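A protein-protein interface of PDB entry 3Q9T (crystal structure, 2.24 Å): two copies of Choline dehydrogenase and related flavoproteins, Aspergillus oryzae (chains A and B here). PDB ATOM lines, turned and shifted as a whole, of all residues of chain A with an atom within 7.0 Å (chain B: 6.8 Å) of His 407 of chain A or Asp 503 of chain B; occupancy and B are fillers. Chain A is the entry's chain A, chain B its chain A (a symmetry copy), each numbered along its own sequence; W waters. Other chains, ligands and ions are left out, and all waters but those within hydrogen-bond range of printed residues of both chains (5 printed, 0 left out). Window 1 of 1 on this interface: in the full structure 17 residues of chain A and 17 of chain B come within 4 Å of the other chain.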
ATOM      1  N   ARG A  79     -13.457  -0.645 -26.879  1.00  0.00           N
ATOM      2  CA  ARG A  79     -12.479  -0.579 -25.806  1.00  0.00           C
ATOM      3  C   ARG A  79     -13.179  -0.609 -24.449  1.00  0.00           C
ATOM      4  O   ARG A  79     -14.216   0.021 -24.253  1.00  0.00           O
ATOM      5  CB  ARG A  79     -11.638   0.681 -25.948  1.00  0.00           C
ATOM      6  CG  ARG A  79     -10.689   0.953 -24.808  1.00  0.00           C
ATOM      7  CD  ARG A  79      -9.474   1.697 -25.331  1.00  0.00           C
ATOM      8  NE  ARG A  79      -9.809   2.981 -25.941  1.00  0.00           N
ATOM      9  CZ  ARG A  79     -10.089   4.081 -25.240  1.00  0.00           C
ATOM     10  NH1 ARG A  79     -10.076   4.049 -23.918  1.00  0.00           N
ATOM     11  NH2 ARG A  79     -10.379   5.215 -25.853  1.00  0.00           N
ATOM     12  N   ILE A  80     -12.608  -1.348 -23.518  1.00  0.00           N
ATOM     13  CA  ILE A  80     -13.133  -1.402 -22.174  1.00  0.00           C
ATOM     14  C   ILE A  80     -12.003  -0.892 -21.298  1.00  0.00           C
ATOM     15  O   ILE A  80     -10.835  -1.095 -21.610  1.00  0.00           O
ATOM     16  CB  ILE A  80     -13.593  -2.819 -21.800  1.00  0.00           C
ATOM     17  CG1 ILE A  80     -14.166  -2.848 -20.376  1.00  0.00           C
ATOM     18  CG2 ILE A  80     -12.440  -3.821 -21.969  1.00  0.00           C
ATOM     19  CD1 ILE A  80     -14.672  -4.251 -19.953  1.00  0.00           C
ATOM     20  N   GLU A  81     -12.341  -0.153 -20.249  1.00  0.00           N
ATOM     21  CA  GLU A  81     -11.309   0.436 -19.399  1.00  0.00           C
ATOM     22  C   GLU A  81     -11.548   0.209 -17.916  1.00  0.00           C
ATOM     23  O   GLU A  81     -12.686  -0.034 -17.470  1.00  0.00           O
ATOM     24  CB  GLU A  81     -11.177   1.940 -19.660  1.00  0.00           C
ATOM     25  CG  GLU A  81     -10.730   2.315 -21.075  1.00  0.00           C
ATOM     26  CD  GLU A  81      -9.225   2.169 -21.289  1.00  0.00           C
ATOM     27  OE1 GLU A  81      -8.501   1.897 -20.313  1.00  0.00           O
ATOM     28  OE2 GLU A  81      -8.763   2.339 -22.441  1.00  0.00           O
ATOM     29  N   LYS A  82     -10.458   0.299 -17.161  1.00  0.00           N
ATOM     30  CA  LYS A  82     -10.516   0.338 -15.716  1.00  0.00           C
ATOM     31  C   LYS A  82      -9.311   1.129 -15.261  1.00  0.00           C
ATOM     32  O   LYS A  82      -8.213   0.879 -15.720  1.00  0.00           O
ATOM     33  CB  LYS A  82     -10.500  -1.077 -15.134  1.00  0.00           C
ATOM     34  CG  LYS A  82     -10.275  -1.151 -13.636  1.00  0.00           C
ATOM     35  CD  LYS A  82     -10.067  -2.591 -13.232  1.00  0.00           C
ATOM     36  CE  LYS A  82      -9.813  -2.737 -11.763  1.00  0.00           C
ATOM     37  NZ  LYS A  82     -10.996  -2.331 -11.012  1.00  0.00           N
ATOM     38  N   THR A 402      -2.459  12.780 -14.995  1.00  0.00           N
ATOM     39  CA  THR A 402      -2.581  11.331 -15.128  1.00  0.00           C
ATOM     40  C   THR A 402      -4.023  10.938 -15.332  1.00  0.00           C
ATOM     41  O   THR A 402      -4.285   9.965 -16.016  1.00  0.00           O
ATOM     42  CB  THR A 402      -2.069  10.580 -13.888  1.00  0.00           C
ATOM     43  OG1 THR A 402      -2.609  11.198 -12.715  1.00  0.00           O
ATOM     44  CG2 THR A 402      -0.540  10.622 -13.829  1.00  0.00           C
ATOM     45  N   PHE A 404      -6.112  12.110 -17.151  1.00  0.00           N
ATOM     46  CA  PHE A 404      -6.546  12.339 -18.527  1.00  0.00           C
ATOM     47  C   PHE A 404      -5.604  11.737 -19.563  1.00  0.00           C
ATOM     48  O   PHE A 404      -5.620  12.141 -20.716  1.00  0.00           O
ATOM     49  CB  PHE A 404      -6.686  13.832 -18.788  1.00  0.00           C
ATOM     50  CG  PHE A 404      -7.717  14.500 -17.931  1.00  0.00           C
ATOM     51  CD1 PHE A 404      -9.065  14.364 -18.221  1.00  0.00           C
ATOM     52  CD2 PHE A 404      -7.339  15.266 -16.831  1.00  0.00           C
ATOM     53  CE1 PHE A 404     -10.022  14.979 -17.443  1.00  0.00           C
ATOM     54  CE2 PHE A 404      -8.310  15.904 -16.044  1.00  0.00           C
ATOM     55  CZ  PHE A 404      -9.649  15.750 -16.361  1.00  0.00           C
ATOM     56  N   GLN A 405      -4.785  10.779 -19.138  1.00  0.00           N
ATOM     57  CA  GLN A 405      -3.776  10.157 -19.994  1.00  0.00           C
ATOM     58  C   GLN A 405      -3.641   8.718 -19.535  1.00  0.00           C
ATOM     59  O   GLN A 405      -2.665   8.335 -18.884  1.00  0.00           O
ATOM     60  CB  GLN A 405      -2.421  10.856 -19.851  1.00  0.00           C
ATOM     61  CG  GLN A 405      -2.351  12.250 -20.429  1.00  0.00           C
ATOM     62  CD  GLN A 405      -2.356  12.272 -21.945  1.00  0.00           C
ATOM     63  OE1 GLN A 405      -1.305  12.361 -22.562  1.00  0.00           O
ATOM     64  NE2 GLN A 405      -3.540  12.210 -22.549  1.00  0.00           N
ATOM     65  N   TRP A 406      -4.642   7.923 -19.864  1.00  0.00           N
ATOM     66  CA  TRP A 406      -4.793   6.616 -19.241  1.00  0.00           C
ATOM     67  C   TRP A 406      -3.777   5.602 -19.760  1.00  0.00           C
ATOM     68  O   TRP A 406      -3.523   4.599 -19.108  1.00  0.00           O
ATOM     69  CB  TRP A 406      -6.213   6.096 -19.459  1.00  0.00           C
ATOM     70  CG  TRP A 406      -7.255   6.829 -18.697  1.00  0.00           C
ATOM     71  CD1 TRP A 406      -7.072   7.872 -17.829  1.00  0.00           C
ATOM     72  CD2 TRP A 406      -8.656   6.566 -18.716  1.00  0.00           C
ATOM     73  NE1 TRP A 406      -8.275   8.272 -17.314  1.00  0.00           N
ATOM     74  CE2 TRP A 406      -9.264   7.488 -17.841  1.00  0.00           C
ATOM     75  CE3 TRP A 406      -9.458   5.637 -19.387  1.00  0.00           C
ATOM     76  CZ2 TRP A 406     -10.632   7.511 -17.621  1.00  0.00           C
ATOM     77  CZ3 TRP A 406     -10.819   5.664 -19.169  1.00  0.00           C
ATOM     78  CH2 TRP A 406     -11.390   6.592 -18.286  1.00  0.00           C
ATOM     79  N   HIS A 407      -3.192   5.844 -20.932  1.00  0.00           N
ATOM     80  CA  HIS A 407      -2.274   4.839 -21.479  1.00  0.00           C
ATOM     81  C   HIS A 407      -0.854   5.304 -21.700  1.00  0.00           C
ATOM     82  O   HIS A 407      -0.040   4.526 -22.171  1.00  0.00           O
ATOM     83  CB  HIS A 407      -2.840   4.199 -22.756  1.00  0.00           C
ATOM     84  CG  HIS A 407      -4.063   3.377 -22.508  1.00  0.00           C
ATOM     85  ND1 HIS A 407      -4.008   2.072 -22.066  1.00  0.00           N
ATOM     86  CD2 HIS A 407      -5.380   3.689 -22.593  1.00  0.00           C
ATOM     87  CE1 HIS A 407      -5.237   1.606 -21.918  1.00  0.00           C
ATOM     88  NE2 HIS A 407      -6.087   2.570 -22.224  1.00  0.00           N
ATOM     89  N   PHE A 408      -0.560   6.562 -21.354  1.00  0.00           N
ATOM     90  CA  PHE A 408       0.775   7.133 -21.548  1.00  0.00           C
ATOM     91  C   PHE A 408       1.491   7.324 -20.229  1.00  0.00           C
ATOM     92  O   PHE A 408       0.892   7.752 -19.251  1.00  0.00           O
ATOM     93  CB  PHE A 408       0.702   8.474 -22.265  1.00  0.00           C
ATOM     94  CG  PHE A 408      -0.148   8.450 -23.509  1.00  0.00           C
ATOM     95  CD1 PHE A 408      -0.209   7.314 -24.302  1.00  0.00           C
ATOM     96  CD2 PHE A 408      -0.899   9.568 -23.878  1.00  0.00           C
ATOM     97  CE1 PHE A 408      -0.992   7.300 -25.464  1.00  0.00           C
ATOM     98  CE2 PHE A 408      -1.688   9.560 -25.021  1.00  0.00           C
ATOM     99  CZ  PHE A 408      -1.730   8.422 -25.818  1.00  0.00           C
ATOM    100  N   PRO A 409       2.785   7.003 -20.194  1.00  0.00           N
ATOM    101  CA  PRO A 409       3.489   7.222 -18.930  1.00  0.00           C
ATOM    102  C   PRO A 409       3.584   8.710 -18.602  1.00  0.00           C
ATOM    103  O   PRO A 409       3.376   9.583 -19.459  1.00  0.00           O
ATOM    104  CB  PRO A 409       4.877   6.613 -19.175  1.00  0.00           C
ATOM    105  CG  PRO A 409       5.021   6.519 -20.651  1.00  0.00           C
ATOM    106  CD  PRO A 409       3.641   6.420 -21.240  1.00  0.00           C
ATOM    107  N   TRP A 487       3.192  11.803 -29.003  1.00  0.00           N
ATOM    108  CA  TRP A 487       3.573  11.889 -30.413  1.00  0.00           C
ATOM    109  C   TRP A 487       2.622  12.890 -31.017  1.00  0.00           C
ATOM    110  O   TRP A 487       1.831  13.480 -30.291  1.00  0.00           O
ATOM    111  CB  TRP A 487       3.453  10.533 -31.121  1.00  0.00           C
ATOM    112  CG  TRP A 487       2.169   9.833 -30.830  1.00  0.00           C
ATOM    113  CD1 TRP A 487       0.930  10.178 -31.278  1.00  0.00           C
ATOM    114  CD2 TRP A 487       1.994   8.665 -30.023  1.00  0.00           C
ATOM    115  NE1 TRP A 487      -0.006   9.299 -30.797  1.00  0.00           N
ATOM    116  CE2 TRP A 487       0.619   8.359 -30.026  1.00  0.00           C
ATOM    117  CE3 TRP A 487       2.862   7.853 -29.296  1.00  0.00           C
ATOM    118  CZ2 TRP A 487       0.086   7.266 -29.320  1.00  0.00           C
ATOM    119  CZ3 TRP A 487       2.337   6.771 -28.601  1.00  0.00           C
ATOM    120  CH2 TRP A 487       0.960   6.488 -28.622  1.00  0.00           C
ATOM    121  N   ASP A 503      -9.410   5.834 -30.080  1.00  0.00           N
ATOM    122  CA  ASP A 503      -8.423   5.109 -29.294  1.00  0.00           C
ATOM    123  C   ASP A 503      -7.896   5.911 -28.115  1.00  0.00           C
ATOM    124  O   ASP A 503      -7.296   5.357 -27.192  1.00  0.00           O
ATOM    125  CB  ASP A 503      -7.261   4.635 -30.174  1.00  0.00           C
ATOM    126  CG  ASP A 503      -6.519   3.479 -29.558  1.00  0.00           C
ATOM    127  OD1 ASP A 503      -7.191   2.548 -29.057  1.00  0.00           O
ATOM    128  OD2 ASP A 503      -5.274   3.505 -29.550  1.00  0.00           O
ATOM    129  N   ARG A 504      -8.121   7.216 -28.140  1.00  0.00           N
ATOM    130  CA  ARG A 504      -7.551   8.081 -27.125  1.00  0.00           C
ATOM    131  C   ARG A 504      -8.594   8.734 -26.235  1.00  0.00           C
ATOM    132  O   ARG A 504      -8.252   9.437 -25.270  1.00  0.00           O
ATOM    133  CB  ARG A 504      -6.757   9.184 -27.797  1.00  0.00           C
ATOM    134  CG  ARG A 504      -5.409   8.769 -28.267  1.00  0.00           C
ATOM    135  CD  ARG A 504      -4.442   9.829 -27.835  1.00  0.00           C
ATOM    136  NE  ARG A 504      -3.897  10.479 -28.992  1.00  0.00           N
ATOM    137  CZ  ARG A 504      -3.083  11.522 -28.954  1.00  0.00           C
ATOM    138  NH1 ARG A 504      -2.752  12.079 -27.795  1.00  0.00           N
ATOM    139  NH2 ARG A 504      -2.627  12.016 -30.097  1.00  0.00           N
ATOM    140  N   CYS A 505      -9.862   8.540 -26.575  1.00  0.00           N
ATOM    141  CA  CYS A 505     -10.926   9.196 -25.836  1.00  0.00           C
ATOM    142  C   CYS A 505     -11.126   8.497 -24.494  1.00  0.00           C
ATOM    143  O   CYS A 505     -10.696   7.359 -24.309  1.00  0.00           O
ATOM    144  CB  CYS A 505     -12.227   9.161 -26.635  1.00  0.00           C
ATOM    145  SG  CYS A 505     -13.010   7.533 -26.655  1.00  0.00           S
ATOM    146  N   VAL B  72      -6.985  -9.811 -22.363  1.00  0.00           N
ATOM    147  CA  VAL B  72      -6.857 -10.142 -20.966  1.00  0.00           C
ATOM    148  C   VAL B  72      -8.093  -9.755 -20.187  1.00  0.00           C
ATOM    149  O   VAL B  72      -8.729  -8.739 -20.470  1.00  0.00           O
ATOM    150  CB  VAL B  72      -5.526  -9.609 -20.330  1.00  0.00           C
ATOM    151  CG1 VAL B  72      -4.786  -8.701 -21.279  1.00  0.00           C
ATOM    152  CG2 VAL B  72      -5.765  -8.961 -18.991  1.00  0.00           C
ATOM    153  N   TYR B  77      -7.426  -5.683 -14.518  1.00  0.00           N
ATOM    154  CA  TYR B  77      -7.209  -5.219 -15.892  1.00  0.00           C
ATOM    155  C   TYR B  77      -8.004  -6.028 -16.931  1.00  0.00           C
ATOM    156  O   TYR B  77      -8.134  -7.246 -16.809  1.00  0.00           O
ATOM    157  CB  TYR B  77      -5.700  -5.218 -16.218  1.00  0.00           C
ATOM    158  CG  TYR B  77      -5.362  -4.640 -17.580  1.00  0.00           C
ATOM    159  CD1 TYR B  77      -5.413  -5.437 -18.722  1.00  0.00           C
ATOM    160  CD2 TYR B  77      -5.009  -3.309 -17.727  1.00  0.00           C
ATOM    161  CE1 TYR B  77      -5.120  -4.927 -19.975  1.00  0.00           C
ATOM    162  CE2 TYR B  77      -4.700  -2.776 -18.994  1.00  0.00           C
ATOM    163  CZ  TYR B  77      -4.760  -3.599 -20.114  1.00  0.00           C
ATOM    164  OH  TYR B  77      -4.479  -3.120 -21.379  1.00  0.00           O
ATOM    165  N   ARG B  79      -8.764  -5.827 -21.420  1.00  0.00           N
ATOM    166  CA  ARG B  79      -8.680  -5.156 -22.706  1.00  0.00           C
ATOM    167  C   ARG B  79      -9.286  -6.033 -23.801  1.00  0.00           C
ATOM    168  O   ARG B  79      -9.089  -7.245 -23.827  1.00  0.00           O
ATOM    169  CB  ARG B  79      -7.229  -4.827 -23.025  1.00  0.00           C
ATOM    170  CG  ARG B  79      -6.984  -4.270 -24.404  1.00  0.00           C
ATOM    171  CD  ARG B  79      -5.786  -3.340 -24.367  1.00  0.00           C
ATOM    172  NE  ARG B  79      -4.559  -4.006 -23.936  1.00  0.00           N
ATOM    173  CZ  ARG B  79      -3.829  -4.793 -24.727  1.00  0.00           C
ATOM    174  NH1 ARG B  79      -4.203  -5.012 -25.977  1.00  0.00           N
ATOM    175  NH2 ARG B  79      -2.725  -5.362 -24.279  1.00  0.00           N
ATOM    176  N   GLU B  81      -9.716  -6.205 -28.082  1.00  0.00           N
ATOM    177  CA  GLU B  81      -9.079  -5.637 -29.268  1.00  0.00           C
ATOM    178  C   GLU B  81      -9.753  -6.043 -30.567  1.00  0.00           C
ATOM    179  O   GLU B  81     -10.450  -7.073 -30.645  1.00  0.00           O
ATOM    180  CB  GLU B  81      -7.598  -6.021 -29.331  1.00  0.00           C
ATOM    181  CG  GLU B  81      -6.741  -5.493 -28.178  1.00  0.00           C
ATOM    182  CD  GLU B  81      -6.345  -4.027 -28.346  1.00  0.00           C
ATOM    183  OE1 GLU B  81      -6.623  -3.446 -29.412  1.00  0.00           O
ATOM    184  OE2 GLU B  81      -5.740  -3.457 -27.409  1.00  0.00           O
ATOM    185  N   HIS B 407      -1.192   0.058 -30.952  1.00  0.00           N
ATOM    186  CA  HIS B 407      -1.676   1.365 -30.492  1.00  0.00           C
ATOM    187  C   HIS B 407      -0.747   2.530 -30.743  1.00  0.00           C
ATOM    188  O   HIS B 407      -1.076   3.644 -30.370  1.00  0.00           O
ATOM    189  CB  HIS B 407      -2.099   1.318 -29.016  1.00  0.00           C
ATOM    190  CG  HIS B 407      -3.299   0.459 -28.777  1.00  0.00           C
ATOM    191  ND1 HIS B 407      -4.589   0.908 -28.971  1.00  0.00           N
ATOM    192  CD2 HIS B 407      -3.406  -0.840 -28.406  1.00  0.00           C
ATOM    193  CE1 HIS B 407      -5.438  -0.068 -28.701  1.00  0.00           C
ATOM    194  NE2 HIS B 407      -4.747  -1.142 -28.364  1.00  0.00           N
ATOM    195  N   PHE B 408       0.402   2.272 -31.379  1.00  0.00           N
ATOM    196  CA  PHE B 408       1.393   3.315 -31.653  1.00  0.00           C
ATOM    197  C   PHE B 408       1.443   3.656 -33.126  1.00  0.00           C
ATOM    198  O   PHE B 408       1.387   2.773 -33.972  1.00  0.00           O
ATOM    199  CB  PHE B 408       2.782   2.887 -31.200  1.00  0.00           C
ATOM    200  CG  PHE B 408       2.822   2.349 -29.793  1.00  0.00           C
ATOM    201  CD1 PHE B 408       1.976   2.856 -28.818  1.00  0.00           C
ATOM    202  CD2 PHE B 408       3.703   1.321 -29.451  1.00  0.00           C
ATOM    203  CE1 PHE B 408       2.024   2.360 -27.508  1.00  0.00           C
ATOM    204  CE2 PHE B 408       3.749   0.814 -28.158  1.00  0.00           C
ATOM    205  CZ  PHE B 408       2.909   1.340 -27.184  1.00  0.00           C
ATOM    206  N   TRP B 487       8.380   5.169 -26.088  1.00  0.00           N
ATOM    207  CA  TRP B 487       8.951   5.744 -24.869  1.00  0.00           C
ATOM    208  C   TRP B 487       9.725   4.620 -24.229  1.00  0.00           C
ATOM    209  O   TRP B 487       9.822   3.549 -24.816  1.00  0.00           O
ATOM    210  CB  TRP B 487       7.863   6.262 -23.919  1.00  0.00           C
ATOM    211  CG  TRP B 487       6.745   5.295 -23.726  1.00  0.00           C
ATOM    212  CD1 TRP B 487       6.788   4.121 -23.038  1.00  0.00           C
ATOM    213  CD2 TRP B 487       5.412   5.416 -24.230  1.00  0.00           C
ATOM    214  NE1 TRP B 487       5.565   3.502 -23.085  1.00  0.00           N
ATOM    215  CE2 TRP B 487       4.702   4.276 -23.808  1.00  0.00           C
ATOM    216  CE3 TRP B 487       4.752   6.374 -24.999  1.00  0.00           C
ATOM    217  CZ2 TRP B 487       3.351   4.062 -24.135  1.00  0.00           C
ATOM    218  CZ3 TRP B 487       3.417   6.165 -25.320  1.00  0.00           C
ATOM    219  CH2 TRP B 487       2.731   5.017 -24.885  1.00  0.00           C
ATOM    220  N   MET B 497       6.323  -2.400 -14.819  1.00  0.00           N
ATOM    221  CA  MET B 497       6.442  -3.440 -15.825  1.00  0.00           C
ATOM    222  C   MET B 497       5.160  -4.263 -15.853  1.00  0.00           C
ATOM    223  O   MET B 497       4.758  -4.768 -16.896  1.00  0.00           O
ATOM    224  CB  MET B 497       7.656  -4.336 -15.558  1.00  0.00           C
ATOM    225  CG  MET B 497       8.973  -3.732 -16.012  1.00  0.00           C
ATOM    226  SD  MET B 497       8.909  -3.186 -17.737  1.00  0.00           S
ATOM    227  CE  MET B 497       8.872  -4.802 -18.557  1.00  0.00           C
ATOM    228  N   HIS B 498       4.536  -4.389 -14.683  1.00  0.00           N
ATOM    229  CA  HIS B 498       3.290  -5.123 -14.529  1.00  0.00           C
ATOM    230  C   HIS B 498       2.199  -4.500 -15.409  1.00  0.00           C
ATOM    231  O   HIS B 498       1.466  -5.204 -16.109  1.00  0.00           O
ATOM    232  CB  HIS B 498       2.876  -5.110 -13.057  1.00  0.00           C
ATOM    233  CG  HIS B 498       1.616  -5.863 -12.775  1.00  0.00           C
ATOM    234  ND1 HIS B 498       1.597  -7.029 -12.040  1.00  0.00           N
ATOM    235  CD2 HIS B 498       0.334  -5.620 -13.131  1.00  0.00           C
ATOM    236  CE1 HIS B 498       0.354  -7.471 -11.957  1.00  0.00           C
ATOM    237  NE2 HIS B 498      -0.431  -6.633 -12.608  1.00  0.00           N
ATOM    238  N   ARG B 499       2.115  -3.174 -15.374  1.00  0.00           N
ATOM    239  CA  ARG B 499       1.160  -2.424 -16.172  1.00  0.00           C
ATOM    240  C   ARG B 499       1.556  -2.448 -17.651  1.00  0.00           C
ATOM    241  O   ARG B 499       0.715  -2.640 -18.533  1.00  0.00           O
ATOM    242  CB  ARG B 499       1.091  -0.982 -15.669  1.00  0.00           C
ATOM    243  CG  ARG B 499       0.278  -0.051 -16.553  1.00  0.00           C
ATOM    244  CD  ARG B 499      -1.219  -0.216 -16.340  1.00  0.00           C
ATOM    245  NE  ARG B 499      -1.994   0.627 -17.251  1.00  0.00           N
ATOM    246  CZ  ARG B 499      -3.320   0.731 -17.224  1.00  0.00           C
ATOM    247  NH1 ARG B 499      -4.018   0.054 -16.325  1.00  0.00           N
ATOM    248  NH2 ARG B 499      -3.943   1.507 -18.094  1.00  0.00           N
ATOM    249  N   ALA B 500       2.841  -2.251 -17.911  1.00  0.00           N
ATOM    250  CA  ALA B 500       3.376  -2.296 -19.269  1.00  0.00           C
ATOM    251  C   ALA B 500       3.055  -3.614 -19.980  1.00  0.00           C
ATOM    252  O   ALA B 500       2.622  -3.611 -21.130  1.00  0.00           O
ATOM    253  CB  ALA B 500       4.888  -2.072 -19.249  1.00  0.00           C
ATOM    254  N   VAL B 501       3.268  -4.737 -19.297  1.00  0.00           N
ATOM    255  CA  VAL B 501       3.028  -6.043 -19.907  1.00  0.00           C
ATOM    256  C   VAL B 501       1.548  -6.222 -20.265  1.00  0.00           C
ATOM    257  O   VAL B 501       1.199  -6.573 -21.393  1.00  0.00           O
ATOM    258  CB  VAL B 501       3.501  -7.178 -18.984  1.00  0.00           C
ATOM    259  CG1 VAL B 501       3.025  -8.513 -19.495  1.00  0.00           C
ATOM    260  CG2 VAL B 501       5.022  -7.161 -18.867  1.00  0.00           C
ATOM    261  N   LEU B 502       0.670  -5.950 -19.308  1.00  0.00           N
ATOM    262  CA  LEU B 502      -0.756  -6.094 -19.552  1.00  0.00           C
ATOM    263  C   LEU B 502      -1.243  -5.149 -20.647  1.00  0.00           C
ATOM    264  O   LEU B 502      -2.072  -5.521 -21.481  1.00  0.00           O
ATOM    265  CB  LEU B 502      -1.570  -5.893 -18.268  1.00  0.00           C
ATOM    266  CG  LEU B 502      -1.241  -6.845 -17.112  1.00  0.00           C
ATOM    267  CD1 LEU B 502      -2.046  -6.480 -15.897  1.00  0.00           C
ATOM    268  CD2 LEU B 502      -1.474  -8.313 -17.498  1.00  0.00           C
ATOM    269  N   ASP B 503      -0.739  -3.931 -20.645  1.00  0.00           N
ATOM    270  CA  ASP B 503      -1.297  -2.909 -21.517  1.00  0.00           C
ATOM    271  C   ASP B 503      -0.712  -2.939 -22.919  1.00  0.00           C
ATOM    272  O   ASP B 503      -1.273  -2.358 -23.851  1.00  0.00           O
ATOM    273  CB  ASP B 503      -1.132  -1.514 -20.904  1.00  0.00           C
ATOM    274  CG  ASP B 503      -2.115  -0.525 -21.472  1.00  0.00           C
ATOM    275  OD1 ASP B 503      -3.308  -0.888 -21.598  1.00  0.00           O
ATOM    276  OD2 ASP B 503      -1.703   0.599 -21.813  1.00  0.00           O
ATOM    277  N   ARG B 504       0.413  -3.619 -23.076  1.00  0.00           N
ATOM    278  CA  ARG B 504       1.114  -3.603 -24.347  1.00  0.00           C
ATOM    279  C   ARG B 504       1.146  -4.957 -25.033  1.00  0.00           C
ATOM    280  O   ARG B 504       1.640  -5.080 -26.166  1.00  0.00           O
ATOM    281  CB  ARG B 504       2.546  -3.161 -24.122  1.00  0.00           C
ATOM    282  CG  ARG B 504       2.716  -1.694 -23.956  1.00  0.00           C
ATOM    283  CD  ARG B 504       3.872  -1.280 -24.815  1.00  0.00           C
ATOM    284  NE  ARG B 504       4.942  -0.809 -23.983  1.00  0.00           N
ATOM    285  CZ  ARG B 504       6.138  -0.458 -24.425  1.00  0.00           C
ATOM    286  NH1 ARG B 504       6.444  -0.573 -25.712  1.00  0.00           N
ATOM    287  NH2 ARG B 504       7.034  -0.014 -23.554  1.00  0.00           N
ATOM    288  N   CYS B 505       0.661  -5.980 -24.340  1.00  0.00           N
ATOM    289  CA  CYS B 505       0.729  -7.326 -24.879  1.00  0.00           C
ATOM    290  C   CYS B 505      -0.326  -7.498 -25.969  1.00  0.00           C
ATOM    291  O   CYS B 505      -1.277  -6.721 -26.050  1.00  0.00           O
ATOM    292  CB  CYS B 505       0.499  -8.353 -23.773  1.00  0.00           C
ATOM    293  SG  CYS B 505      -1.226  -8.465 -23.248  1.00  0.00           S
HETATM  294  O   HOH W   1       0.517   1.773 -22.789  1.00  0.00           O
HETATM  295  O   HOH W   2      -7.281  -1.243 -20.451  1.00  0.00           O
HETATM  296  O   HOH W   3      -7.099   2.627 -17.772  1.00  0.00           O
HETATM  297  O   HOH W   4      -6.421   0.286 -18.583  1.00  0.00           O
HETATM  298  O   HOH W   5      -3.248   5.276 -29.427  1.00  0.00           O
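O of Trp 406 of chain A lies within hydrogen-bond range of NH2 of Arg 499 of chain B. OD2 of Asp 503 of chain B is in hydrogen-bond range of ND1 of His 407 of chain A. OD2 of Asp 503 of chain A lies within hydrogen-bond range of ND1 of His 407 of chain B, 2.7 Å away.
NH2 of Arg 79 of chain A lies within hydrogen-bond range of O of Asp 503 of chain A. The side-chain carboxylate of Glu 81 of chain A is in hydrogen-bond range of a ring nitrogen (NE2) of His 407 of chain A (2.7 Å). The side-chain hydroxyl (OH) of Tyr 77 of chain B is in hydrogen-bond range of the side-chain carboxylate (OD1) of Asp 503 of chain B, 2.5 Å away. The backbone carbonyl oxygen of Asp 503 of chain B lies within hydrogen-bond range of the guanidinium group of Arg 79 of chain B (3.4 Å). OE2 of Glu 81 of chain B sits at hydrogen-bond distance from NE2 of His 407 of chain B.
Among the printed residues, merely in contact across the chains: Trp 487 of chain A with Trp 487 of chain B (3.5 Å), Pro 409 of chain A with Trp 487 of chain B (3.5 Å), Phe 408 of chain A with Trp 487 of chain B (3.8 Å), Trp 487 of chain A with Phe 408 of chain B (3.8 Å), His 407 of chain A with Trp 487 of chain B (3.9 Å) and Trp 487 of chain A with His 407 of chain B (3.9 Å).
Printed residues of chain B within 4 Å of His 407 of chain A: Trp 487 and Asp 503. Of the printed residues of chain B, Trp 487 of chain A touches His 407 (3.9 Å), Phe 408 (3.8 Å) and Trp 487 (3.5 Å). Printed residues of chain A within 4 Å of His 407 of chain B: Trp 487 and Asp 503. Of the printed residues of chain A, Phe 408 of chain B touches Trp 487. Printed residues of chain A within 4 Å of Trp 487 of chain B: His 407 (3.9 Å), Phe 408 (3.8 Å), Pro 409 (3.5 Å) and Trp 487 (3.5 Å). Asp 503 of chain B touches just one residue of chain A: His 407 (2.7 Å). Cys 505 of chain B touches none of the printed residues of chain A. The nearest printed residue of chain B that does not touch His 407 of chain A is Arg 499 of chain B (4.01 Å). The nearest residue of chain A that does not touch Asp 503 of chain B is Trp 406 of chain A (5.2 Å). The nearest printed residue of chain B that does not touch Trp 487 of chain A is Arg 504 of chain B (8.9 Å).
Of the 15 printed residues of chain A, 6 touch a printed residue of chain B. Hydrophobic or aromatic side chains of chain A that line the printed part of chain B: His 407, Phe 408, Pro 409 and Trp 487. Along chain B the printed residues that touch a printed residue of chain A span positions 407 to 503. Among the printed residues, no Asp or Glu carboxylate lies within 4 Å of a Lys or Arg side-chain nitrogen of the other chain.
His 407 of chain A touches Trp 487 of chain B, and with the chains exchanged Trp 487 of chain A touches His 407 of chain B. His 407 of chain A touches Asp 503 of chain B, and with the chains exchanged Asp 503 of chain A touches His 407 of chain B. Phe 408 of chain A touches Trp 487 of chain B, and with the chains exchanged Trp 487 of chain A touches Phe 408 of chain B. Trp 487 of chain B touches its own counterpart, Trp 487 of chain A.
Water W1 lies within hydrogen-bond range of OD2 of Asp 503 of chain B and O of His 407 of chain A. Water W5 bridges the side-chain carboxylate of Asp 503 of chain A (2.7 Å) and the backbone carbonyl oxygen of His 407 of chain B (2.9 Å). Water W3 lies within hydrogen-bond range of the backbone carbonyl oxygen (O) of Lys 82 of chain A, the side-chain carboxylate (OE1) of Glu 81 of chain A and the guanidinium group (NH2) of Arg 499 of chain B. Water W2 lies within hydrogen-bond range of the side-chain carboxylate of Glu 81 of chain A (3.4 Å) and the side-chain hydroxyl of Tyr 77 of chain B (3.5 Å).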
